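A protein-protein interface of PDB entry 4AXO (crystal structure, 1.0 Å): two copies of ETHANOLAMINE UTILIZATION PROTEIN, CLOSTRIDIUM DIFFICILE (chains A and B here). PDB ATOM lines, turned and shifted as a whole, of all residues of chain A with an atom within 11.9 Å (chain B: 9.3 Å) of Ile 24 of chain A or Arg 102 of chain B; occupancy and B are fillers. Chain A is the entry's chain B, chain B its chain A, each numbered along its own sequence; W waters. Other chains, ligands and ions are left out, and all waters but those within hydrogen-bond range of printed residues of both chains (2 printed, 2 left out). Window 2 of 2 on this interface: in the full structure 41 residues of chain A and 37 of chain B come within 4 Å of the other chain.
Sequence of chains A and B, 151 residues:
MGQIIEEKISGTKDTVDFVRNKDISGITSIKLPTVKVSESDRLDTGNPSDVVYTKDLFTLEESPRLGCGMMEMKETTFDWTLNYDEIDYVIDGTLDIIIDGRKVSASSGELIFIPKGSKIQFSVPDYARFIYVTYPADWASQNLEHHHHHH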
ATOM      1  N   ARG A  20     -29.891 -23.142   4.317  1.00  0.00           N
ATOM      2  CA  ARG A  20     -29.003 -23.361   5.457  1.00  0.00           C
ATOM      3  C   ARG A  20     -28.217 -22.086   5.720  1.00  0.00           C
ATOM      4  O   ARG A  20     -28.087 -21.223   4.852  1.00  0.00           O
ATOM      5  CB  ARG A  20     -28.059 -24.554   5.239  1.00  0.00           C
ATOM      6  CG  ARG A  20     -26.986 -24.297   4.185  1.00  0.00           C
ATOM      7  CD  ARG A  20     -26.012 -25.428   4.066  1.00  0.00           C
ATOM      8  NE  ARG A  20     -25.025 -25.139   3.029  1.00  0.00           N
ATOM      9  CZ  ARG A  20     -24.036 -25.951   2.685  1.00  0.00           C
ATOM     10  NH1 ARG A  20     -23.829 -27.074   3.340  1.00  0.00           N
ATOM     11  NH2 ARG A  20     -23.212 -25.603   1.704  1.00  0.00           N
ATOM     12  N   ASN A  21     -27.659 -21.988   6.923  1.00  0.00           N
ATOM     13  CA  ASN A  21     -26.668 -20.989   7.258  1.00  0.00           C
ATOM     14  C   ASN A  21     -25.428 -21.726   7.735  1.00  0.00           C
ATOM     15  O   ASN A  21     -25.398 -22.208   8.876  1.00  0.00           O
ATOM     16  CB  ASN A  21     -27.191 -20.045   8.328  1.00  0.00           C
ATOM     17  CG  ASN A  21     -26.156 -19.039   8.740  1.00  0.00           C
ATOM     18  OD1 ASN A  21     -25.196 -18.804   8.006  1.00  0.00           O
ATOM     19  ND2 ASN A  21     -26.322 -18.459   9.908  1.00  0.00           N
ATOM     20  N   LYS A  22     -24.461 -21.865   6.837  1.00  0.00           N
ATOM     21  CA  LYS A  22     -23.207 -22.526   7.168  1.00  0.00           C
ATOM     22  C   LYS A  22     -22.209 -21.471   7.578  1.00  0.00           C
ATOM     23  O   LYS A  22     -21.702 -20.704   6.748  1.00  0.00           O
ATOM     24  CB  LYS A  22     -22.718 -23.291   5.956  1.00  0.00           C
ATOM     25  CG  LYS A  22     -21.421 -24.017   6.149  1.00  0.00           C
ATOM     26  CD  LYS A  22     -21.054 -24.778   4.872  1.00  0.00           C
ATOM     27  CE  LYS A  22     -19.668 -25.323   4.884  1.00  0.00           C
ATOM     28  NZ  LYS A  22     -19.376 -26.016   3.602  1.00  0.00           N
ATOM     29  N   ASP A  23     -21.950 -21.394   8.865  1.00  0.00           N
ATOM     30  CA  ASP A  23     -21.028 -20.403   9.416  1.00  0.00           C
ATOM     31  C   ASP A  23     -19.586 -20.747   9.106  1.00  0.00           C
ATOM     32  O   ASP A  23     -19.239 -21.913   8.899  1.00  0.00           O
ATOM     33  CB  ASP A  23     -21.243 -20.365  10.930  1.00  0.00           C
ATOM     34  CG  ASP A  23     -20.434 -19.270  11.619  1.00  0.00           C
ATOM     35  OD1 ASP A  23     -20.844 -18.094  11.498  1.00  0.00           O
ATOM     36  OD2 ASP A  23     -19.416 -19.593  12.290  1.00  0.00           O
ATOM     37  N   ILE A  24     -18.754 -19.709   9.112  1.00  0.00           N
ATOM     38  CA  ILE A  24     -17.326 -19.840   8.944  1.00  0.00           C
ATOM     39  C   ILE A  24     -16.764 -20.970   9.854  1.00  0.00           C
ATOM     40  O   ILE A  24     -15.859 -21.697   9.496  1.00  0.00           O
ATOM     41  CB  ILE A  24     -16.657 -18.447   9.246  1.00  0.00           C
ATOM     42  CG1 ILE A  24     -16.944 -17.457   8.100  1.00  0.00           C
ATOM     43  CG2 ILE A  24     -15.200 -18.599   9.555  1.00  0.00           C
ATOM     44  CD1 ILE A  24     -16.738 -15.952   8.498  1.00  0.00           C
ATOM     45  N   SER A  25     -17.286 -21.102  11.061  1.00  0.00           N
ATOM     46  CA  SER A  25     -16.798 -22.095  12.048  1.00  0.00           C
ATOM     47  C   SER A  25     -17.203 -23.548  11.758  1.00  0.00           C
ATOM     48  O   SER A  25     -16.785 -24.474  12.481  1.00  0.00           O
ATOM     49  CB  SER A  25     -17.394 -21.777  13.414  1.00  0.00           C
ATOM     50  OG  SER A  25     -18.813 -21.977  13.344  1.00  0.00           O
ATOM     51  N   GLY A  26     -18.084 -23.748  10.784  1.00  0.00           N
ATOM     52  CA  GLY A  26     -18.667 -25.058  10.541  1.00  0.00           C
ATOM     53  C   GLY A  26     -20.040 -25.254  11.188  1.00  0.00           C
ATOM     54  O   GLY A  26     -20.786 -26.160  10.777  1.00  0.00           O
ATOM     55  N   ILE A  27     -20.363 -24.462  12.197  1.00  0.00           N
ATOM     56  CA  ILE A  27     -21.688 -24.504  12.799  1.00  0.00           C
ATOM     57  C   ILE A  27     -22.709 -24.165  11.708  1.00  0.00           C
ATOM     58  O   ILE A  27     -22.544 -23.182  10.984  1.00  0.00           O
ATOM     59  CB  ILE A  27     -21.779 -23.569  13.998  1.00  0.00           C
ATOM     60  CG1 ILE A  27     -20.816 -23.996  15.074  1.00  0.00           C
ATOM     61  CG2 ILE A  27     -23.214 -23.492  14.499  1.00  0.00           C
ATOM     62  CD1 ILE A  27     -20.781 -23.089  16.296  1.00  0.00           C
ATOM     63  N   THR A  28     -23.761 -24.978  11.567  1.00  0.00           N
ATOM     64  CA  THR A  28     -24.689 -24.857  10.465  1.00  0.00           C
ATOM     65  C   THR A  28     -26.109 -25.042  10.925  1.00  0.00           C
ATOM     66  O   THR A  28     -26.422 -26.086  11.508  1.00  0.00           O
ATOM     67  CB  THR A  28     -24.397 -25.909   9.380  1.00  0.00           C
ATOM     68  OG1 THR A  28     -23.061 -25.761   8.910  1.00  0.00           O
ATOM     69  CG2 THR A  28     -25.307 -25.814   8.197  1.00  0.00           C
ATOM     70  N   SER A  29     -26.996 -24.089  10.619  1.00  0.00           N
ATOM     71  CA  SER A  29     -28.419 -24.314  10.788  1.00  0.00           C
ATOM     72  C   SER A  29     -29.019 -24.754   9.453  1.00  0.00           C
ATOM     73  O   SER A  29     -28.542 -24.343   8.393  1.00  0.00           O
ATOM     74  CB  SER A  29     -29.134 -23.048  11.274  1.00  0.00           C
ATOM     75  OG  SER A  29     -28.949 -21.951  10.408  1.00  0.00           O
ATOM     76  N   PHE A  58     -24.904 -33.185   5.055  1.00  0.00           N
ATOM     77  CA  PHE A  58     -23.536 -32.749   5.354  1.00  0.00           C
ATOM     78  C   PHE A  58     -22.555 -33.606   4.577  1.00  0.00           C
ATOM     79  O   PHE A  58     -22.685 -34.821   4.570  1.00  0.00           O
ATOM     80  CB  PHE A  58     -23.238 -32.860   6.853  1.00  0.00           C
ATOM     81  CG  PHE A  58     -24.098 -31.994   7.696  1.00  0.00           C
ATOM     82  CD1 PHE A  58     -25.336 -32.449   8.132  1.00  0.00           C
ATOM     83  CD2 PHE A  58     -23.722 -30.722   8.022  1.00  0.00           C
ATOM     84  CE1 PHE A  58     -26.163 -31.642   8.867  1.00  0.00           C
ATOM     85  CE2 PHE A  58     -24.534 -29.912   8.760  1.00  0.00           C
ATOM     86  CZ  PHE A  58     -25.768 -30.372   9.182  1.00  0.00           C
ATOM     87  N   GLU A  61     -16.421 -33.629   4.825  1.00  0.00           N
ATOM     88  CA  GLU A  61     -15.596 -32.500   5.245  1.00  0.00           C
ATOM     89  C   GLU A  61     -16.370 -31.615   6.217  1.00  0.00           C
ATOM     90  O   GLU A  61     -15.827 -31.133   7.188  1.00  0.00           O
ATOM     91  CB  GLU A  61     -15.114 -31.706   4.026  1.00  0.00           C
ATOM     92  CG  GLU A  61     -14.141 -30.621   4.373  1.00  0.00           C
ATOM     93  CD  GLU A  61     -14.787 -29.324   4.761  1.00  0.00           C
ATOM     94  OE1 GLU A  61     -15.941 -29.097   4.362  1.00  0.00           O
ATOM     95  OE2 GLU A  61     -14.125 -28.512   5.448  1.00  0.00           O
ATOM     96  N   GLU A  62     -17.657 -31.424   5.971  1.00  0.00           N
ATOM     97  CA  GLU A  62     -18.497 -30.601   6.844  1.00  0.00           C
ATOM     98  C   GLU A  62     -18.718 -31.243   8.209  1.00  0.00           C
ATOM     99  O   GLU A  62     -18.777 -30.543   9.232  1.00  0.00           O
ATOM    100  CB  GLU A  62     -19.846 -30.314   6.185  1.00  0.00           C
ATOM    101  CG  GLU A  62     -19.753 -29.282   5.070  1.00  0.00           C
ATOM    102  CD  GLU A  62     -20.964 -29.206   4.163  1.00  0.00           C
ATOM    103  OE1 GLU A  62     -21.792 -30.124   4.162  1.00  0.00           O
ATOM    104  OE2 GLU A  62     -21.048 -28.230   3.384  1.00  0.00           O
ATOM    105  N   SER A  63     -18.933 -32.547   8.225  1.00  0.00           N
ATOM    106  CA  SER A  63     -19.216 -33.268   9.451  1.00  0.00           C
ATOM    107  C   SER A  63     -18.545 -34.648   9.387  1.00  0.00           C
ATOM    108  O   SER A  63     -19.133 -35.612   8.907  1.00  0.00           O
ATOM    109  CB  SER A  63     -20.719 -33.390   9.707  1.00  0.00           C
ATOM    110  OG  SER A  63     -20.939 -34.002  10.962  1.00  0.00           O
ATOM    111  N   ASP B  96     -30.492 -19.881  19.626  1.00  0.00           N
ATOM    112  CA  ASP B  96     -29.406 -19.165  18.974  1.00  0.00           C
ATOM    113  C   ASP B  96     -28.082 -19.740  19.485  1.00  0.00           C
ATOM    114  O   ASP B  96     -27.943 -20.041  20.671  1.00  0.00           O
ATOM    115  CB  ASP B  96     -29.463 -17.663  19.318  1.00  0.00           C
ATOM    116  CG  ASP B  96     -30.710 -16.930  18.818  1.00  0.00           C
ATOM    117  OD1 ASP B  96     -31.292 -17.316  17.780  1.00  0.00           O
ATOM    118  OD2 ASP B  96     -31.081 -15.923  19.469  1.00  0.00           O
ATOM    119  N   ILE B  97     -27.128 -19.890  18.576  1.00  0.00           N
ATOM    120  CA  ILE B  97     -25.771 -20.304  18.912  1.00  0.00           C
ATOM    121  C   ILE B  97     -24.863 -19.146  18.526  1.00  0.00           C
ATOM    122  O   ILE B  97     -24.856 -18.738  17.371  1.00  0.00           O
ATOM    123  CB  ILE B  97     -25.371 -21.598  18.186  1.00  0.00           C
ATOM    124  CG1 ILE B  97     -26.343 -22.757  18.499  1.00  0.00           C
ATOM    125  CG2 ILE B  97     -23.937 -21.962  18.487  1.00  0.00           C
ATOM    126  CD1 ILE B  97     -26.370 -23.173  19.960  1.00  0.00           C
ATOM    127  N   ILE B  98     -24.106 -18.615  19.480  1.00  0.00           N
ATOM    128  CA  ILE B  98     -23.194 -17.504  19.219  1.00  0.00           C
ATOM    129  C   ILE B  98     -21.783 -18.058  19.167  1.00  0.00           C
ATOM    130  O   ILE B  98     -21.329 -18.719  20.110  1.00  0.00           O
ATOM    131  CB  ILE B  98     -23.283 -16.420  20.305  1.00  0.00           C
ATOM    132  CG1 ILE B  98     -24.750 -16.151  20.691  1.00  0.00           C
ATOM    133  CG2 ILE B  98     -22.560 -15.160  19.854  1.00  0.00           C
ATOM    134  CD1 ILE B  98     -25.579 -15.631  19.551  1.00  0.00           C
ATOM    135  N   ILE B  99     -21.095 -17.795  18.057  1.00  0.00           N
ATOM    136  CA  ILE B  99     -19.771 -18.305  17.797  1.00  0.00           C
ATOM    137  C   ILE B  99     -18.951 -17.161  17.216  1.00  0.00           C
ATOM    138  O   ILE B  99     -19.306 -16.618  16.175  1.00  0.00           O
ATOM    139  CB  ILE B  99     -19.895 -19.502  16.747  1.00  0.00           C
ATOM    140  CG1 ILE B  99     -18.574 -19.961  16.224  1.00  0.00           C
ATOM    141  CG2 ILE B  99     -20.902 -19.198  15.594  1.00  0.00           C
ATOM    142  CD1 ILE B  99     -17.748 -20.361  17.272  1.00  0.00           C
ATOM    143  N   ASP B 100     -17.855 -16.795  17.877  1.00  0.00           N
ATOM    144  CA  ASP B 100     -16.923 -15.801  17.316  1.00  0.00           C
ATOM    145  C   ASP B 100     -17.661 -14.526  16.854  1.00  0.00           C
ATOM    146  O   ASP B 100     -17.399 -13.992  15.782  1.00  0.00           O
ATOM    147  CB  ASP B 100     -16.112 -16.425  16.175  1.00  0.00           C
ATOM    148  CG  ASP B 100     -14.903 -15.625  15.763  1.00  0.00           C
ATOM    149  OD1 ASP B 100     -14.328 -14.875  16.572  1.00  0.00           O
ATOM    150  OD2 ASP B 100     -14.516 -15.808  14.587  1.00  0.00           O
ATOM    151  N   GLY B 101     -18.620 -14.098  17.659  1.00  0.00           N
ATOM    152  CA  GLY B 101     -19.355 -12.883  17.401  1.00  0.00           C
ATOM    153  C   GLY B 101     -20.421 -12.975  16.325  1.00  0.00           C
ATOM    154  O   GLY B 101     -20.966 -11.937  15.922  1.00  0.00           O
ATOM    155  N   ARG B 102     -20.726 -14.177  15.854  1.00  0.00           N
ATOM    156  CA  ARG B 102     -21.719 -14.454  14.814  1.00  0.00           C
ATOM    157  C   ARG B 102     -22.819 -15.319  15.405  1.00  0.00           C
ATOM    158  O   ARG B 102     -22.601 -16.035  16.370  1.00  0.00           O
ATOM    159  CB  ARG B 102     -21.075 -15.131  13.615  1.00  0.00           C
ATOM    160  CG  ARG B 102     -19.979 -14.278  12.975  1.00  0.00           C
ATOM    161  CD  ARG B 102     -19.364 -14.897  11.719  1.00  0.00           C
ATOM    162  NE  ARG B 102     -18.811 -16.205  12.019  1.00  0.00           N
ATOM    163  CZ  ARG B 102     -17.624 -16.462  12.545  1.00  0.00           C
ATOM    164  NH1 ARG B 102     -16.692 -15.520  12.628  1.00  0.00           N
ATOM    165  NH2 ARG B 102     -17.365 -17.685  12.996  1.00  0.00           N
ATOM    166  N   LYS B 103     -23.994 -15.270  14.809  1.00  0.00           N
ATOM    167  CA  LYS B 103     -25.149 -15.991  15.311  1.00  0.00           C
ATOM    168  C   LYS B 103     -25.686 -16.984  14.276  1.00  0.00           C
ATOM    169  O   LYS B 103     -25.869 -16.634  13.104  1.00  0.00           O
ATOM    170  CB  LYS B 103     -26.253 -14.996  15.675  1.00  0.00           C
ATOM    171  CG  LYS B 103     -27.497 -15.598  16.281  1.00  0.00           C
ATOM    172  CD  LYS B 103     -28.553 -14.540  16.619  1.00  0.00           C
ATOM    173  CE  LYS B 103     -28.148 -13.657  17.760  1.00  0.00           C
ATOM    174  NZ  LYS B 103     -29.147 -12.547  17.889  1.00  0.00           N
ATOM    175  N   VAL B 104     -25.956 -18.196  14.728  1.00  0.00           N
ATOM    176  CA  VAL B 104     -26.603 -19.236  13.951  1.00  0.00           C
ATOM    177  C   VAL B 104     -27.862 -19.611  14.743  1.00  0.00           C
ATOM    178  O   VAL B 104     -27.754 -19.891  15.925  1.00  0.00           O
ATOM    179  CB  VAL B 104     -25.663 -20.443  13.786  1.00  0.00           C
ATOM    180  CG1 VAL B 104     -26.377 -21.554  13.047  1.00  0.00           C
ATOM    181  CG2 VAL B 104     -24.381 -20.045  13.068  1.00  0.00           C
ATOM    182  N   SER B 105     -29.025 -19.655  14.094  1.00  0.00           N
ATOM    183  CA  SER B 105     -30.302 -19.815  14.789  1.00  0.00           C
ATOM    184  C   SER B 105     -31.159 -20.896  14.170  1.00  0.00           C
ATOM    185  O   SER B 105     -31.116 -21.111  12.960  1.00  0.00           O
ATOM    186  CB  SER B 105     -31.095 -18.512  14.730  1.00  0.00           C
ATOM    187  OG  SER B 105     -30.374 -17.460  15.322  1.00  0.00           O
ATOM    188  N   PRO B 115     -19.702 -28.482  15.454  1.00  0.00           N
ATOM    189  CA  PRO B 115     -18.532 -29.366  15.488  1.00  0.00           C
ATOM    190  C   PRO B 115     -17.887 -29.428  16.856  1.00  0.00           C
ATOM    191  O   PRO B 115     -17.862 -28.455  17.639  1.00  0.00           O
ATOM    192  CB  PRO B 115     -17.554 -28.705  14.520  1.00  0.00           C
ATOM    193  CG  PRO B 115     -18.245 -27.718  13.796  1.00  0.00           C
ATOM    194  CD  PRO B 115     -19.490 -27.361  14.536  1.00  0.00           C
ATOM    195  N   SER B 118     -16.045 -26.489  19.402  1.00  0.00           N
ATOM    196  CA  SER B 118     -16.623 -25.162  19.265  1.00  0.00           C
ATOM    197  C   SER B 118     -16.813 -24.507  20.622  1.00  0.00           C
ATOM    198  O   SER B 118     -17.378 -25.109  21.542  1.00  0.00           O
ATOM    199  CB  SER B 118     -17.983 -25.275  18.578  1.00  0.00           C
ATOM    200  OG  SER B 118     -17.900 -25.775  17.273  1.00  0.00           O
ATOM    201  N   LYS B 119     -16.370 -23.262  20.712  1.00  0.00           N
ATOM    202  CA  LYS B 119     -16.543 -22.401  21.882  1.00  0.00           C
ATOM    203  C   LYS B 119     -17.725 -21.520  21.576  1.00  0.00           C
ATOM    204  O   LYS B 119     -17.640 -20.624  20.733  1.00  0.00           O
ATOM    205  CB  LYS B 119     -15.345 -21.488  22.089  1.00  0.00           C
ATOM    206  CG  LYS B 119     -14.080 -22.209  22.276  1.00  0.00           C
ATOM    207  CD  LYS B 119     -12.935 -21.249  22.534  1.00  0.00           C
ATOM    208  CE  LYS B 119     -13.064 -20.578  23.903  1.00  0.00           C
ATOM    209  NZ  LYS B 119     -12.008 -19.553  24.180  1.00  0.00           N
ATOM    210  N   ILE B 120     -18.843 -21.761  22.244  1.00  0.00           N
ATOM    211  CA  ILE B 120     -20.099 -21.116  21.870  1.00  0.00           C
ATOM    212  C   ILE B 120     -20.760 -20.500  23.054  1.00  0.00           C
ATOM    213  O   ILE B 120     -20.378 -20.682  24.224  1.00  0.00           O
ATOM    214  CB  ILE B 120     -21.090 -22.136  21.239  1.00  0.00           C
ATOM    215  CG1 ILE B 120     -21.600 -23.193  22.258  1.00  0.00           C
ATOM    216  CG2 ILE B 120     -20.476 -22.800  20.030  1.00  0.00           C
ATOM    217  CD1 ILE B 120     -22.826 -23.930  21.765  1.00  0.00           C
ATOM    218  N   GLN B 121     -21.813 -19.744  22.769  1.00  0.00           N
ATOM    219  CA  GLN B 121     -22.857 -19.485  23.744  1.00  0.00           C
ATOM    220  C   GLN B 121     -24.128 -20.139  23.241  1.00  0.00           C
ATOM    221  O   GLN B 121     -24.511 -19.961  22.092  1.00  0.00           O
ATOM    222  CB  GLN B 121     -23.103 -18.011  23.966  1.00  0.00           C
ATOM    223  CG  GLN B 121     -21.850 -17.289  24.487  1.00  0.00           C
ATOM    224  CD  GLN B 121     -22.007 -15.810  24.451  1.00  0.00           C
ATOM    225  OE1 GLN B 121     -22.592 -15.196  25.352  1.00  0.00           O
ATOM    226  NE2 GLN B 121     -21.444 -15.216  23.422  1.00  0.00           N
ATOM    227  N   SER B 123     -27.780 -19.533  23.430  1.00  0.00           N
ATOM    228  CA  SER B 123     -28.488 -18.288  23.709  1.00  0.00           C
ATOM    229  C   SER B 123     -29.971 -18.434  23.392  1.00  0.00           C
ATOM    230  O   SER B 123     -30.353 -18.652  22.247  1.00  0.00           O
ATOM    231  CB  SER B 123     -27.865 -17.147  22.935  1.00  0.00           C
ATOM    232  OG  SER B 123     -28.500 -15.916  23.245  1.00  0.00           O
HETATM  233  O   HOH W   1     -28.827 -19.292  11.260  1.00  0.00           O
HETATM  234  O   HOH W   2     -16.134 -24.900  15.300  1.00  0.00           O
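OD1 of Asp 23 of chain A is in salt-bridge range of NE of Arg 102 of chain B.
The backbone carbonyl oxygen (O) of Ser 105 of chain B sits close to the side-chain hydroxyl (OG) of Ser 29 of chain A (3.5 Å).
NH1 of Arg 102 of chain B is in salt-bridge range of OD2 of Asp 100 of chain B (2.9 Å).
The side-chain hydroxyl (OG) of Ser 105 of chain B lies within hydrogen-bond range of the side-chain carboxylate (OD1) of Asp 96 of chain B, 2.6 Å away.
The backbone NH of Asn 21 of chain A is in hydrogen-bond range of the backbone carbonyl oxygen of Ser 29 of chain A (2.9 Å).
The side-chain hydroxyl (OG1) of Thr 28 of chain A lies within hydrogen-bond range of the backbone carbonyl oxygen (O) of Gly 26 of chain A, 3.0 Å away.
The side-chain carboxylate of Asp 23 of chain A sits at hydrogen-bond distance from the side-chain hydroxyl of Ser 25 of chain A.
The side-chain hydroxyl (OG) of Ser 118 of chain B sits at hydrogen-bond distance from the backbone carbonyl oxygen (O) of Pro 115 of chain B (2.7 Å).
Among the printed residues, pairs that only touch across the chains: Ser 25 of chain A with Ile 99 of chain B (3.5 Å), Ser 29 of chain A with Val 104 of chain B (3.6 Å), Asp 23 of chain A with Ile 99 of chain B (3.6 Å), Ile 27 of chain A with Pro 115 of chain B (3.7 Å), Asn 21 of chain A with Lys 103 of chain B (3.7 Å), Ile 27 of chain A with Ile 99 of chain B (3.7 Å), Ile 27 of chain A with Ile 120 of chain B (3.8 Å), Ser 25 of chain A with Pro 115 of chain B (3.8 Å), Asp 23 of chain A with Val 104 of chain B (3.8 Å), Ile 24 of chain A with Arg 102 of chain B (3.9 Å), Ile 27 of chain A with Val 104 of chain B (3.9 Å), Ser 25 of chain A with Arg 102 of chain B (3.9 Å) and Gly 26 of chain A with Pro 115 of chain B (3.99 Å).
Of the printed residues of chain B, Asp 23 of chain A touches Ile 99 (3.6 Å), Arg 102 (2.8 Å) and Val 104 (3.8 Å).
Of the printed residues of chain B, Ile 24 of chain A touches Arg 102 (3.9 Å).
Ser 25 of chain A touches just these residues of chain B: Ile 99 (3.5 Å), Arg 102 (3.9 Å) and Pro 115 (3.8 Å).
Of the printed residues of chain B, Gly 26 of chain A touches Pro 115 (3.99 Å).
Of chain A, only Asp 23, Ser 25 and Ile 27 come within 4 Å of Ile 99 of chain B.
No residue of chain A comes within 4 Å of Gly 101 of chain B.
Printed residues of chain A within 4 Å of Arg 102 of chain B: Asp 23 (2.8 Å), Ile 24 (3.9 Å) and Ser 25 (3.9 Å).
Of chain A, only Asp 23, Ile 27 and Ser 29 come within 4 Å of Val 104 of chain B.
Printed residues of chain A within 4 Å of Ile 120 of chain B: Ile 27.
Gln 121 of chain B touches none of the printed residues of chain A.
Ser 123 of chain B touches none of the printed residues of chain A.
The nearest residue of chain B that does not touch Ile 24 of chain A is Asp 100 of chain B (5.8 Å).
Of the 14 printed residues of chain A, 7 touch a printed residue of chain B.
Printed residues of chain B that touch a printed residue of chain A: Ile 99, Arg 102, Lys 103, Val 104, Ser 105, Pro 115 and Ile 120.
Hydrophobic or aromatic side chains of chain B within 4 Å of the printed part of chain A: Ile 99, Val 104, Pro 115 and Ile 120.
Along chain B the printed residues that touch a printed residue of chain A span positions 99 to 120.
Among the printed residues, Asp or Glu carboxylates within 4 Å of a Lys or Arg side-chain nitrogen of the other chain: Asp 23 of chain A with Arg 102 of chain B (2.8 Å).
No position is printed for both chains.
Of the 15 pairs that touch across the chains among the printed residues, none has its exchanged pair printed and touching as well.
Water W2 lies within hydrogen-bond range of the side-chain hydroxyl of Ser 118 of chain B and the backbone carbonyl oxygen of Ser 25 of chain A.
Water W1 lies within hydrogen-bond range of the side-chain hydroxyl of Ser 29 of chain A (2.8 Å), the backbone NH of Ser 105 of chain B (2.9 Å) and the side-chain amide nitrogen of Asn 21 of chain A (3.0 Å).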
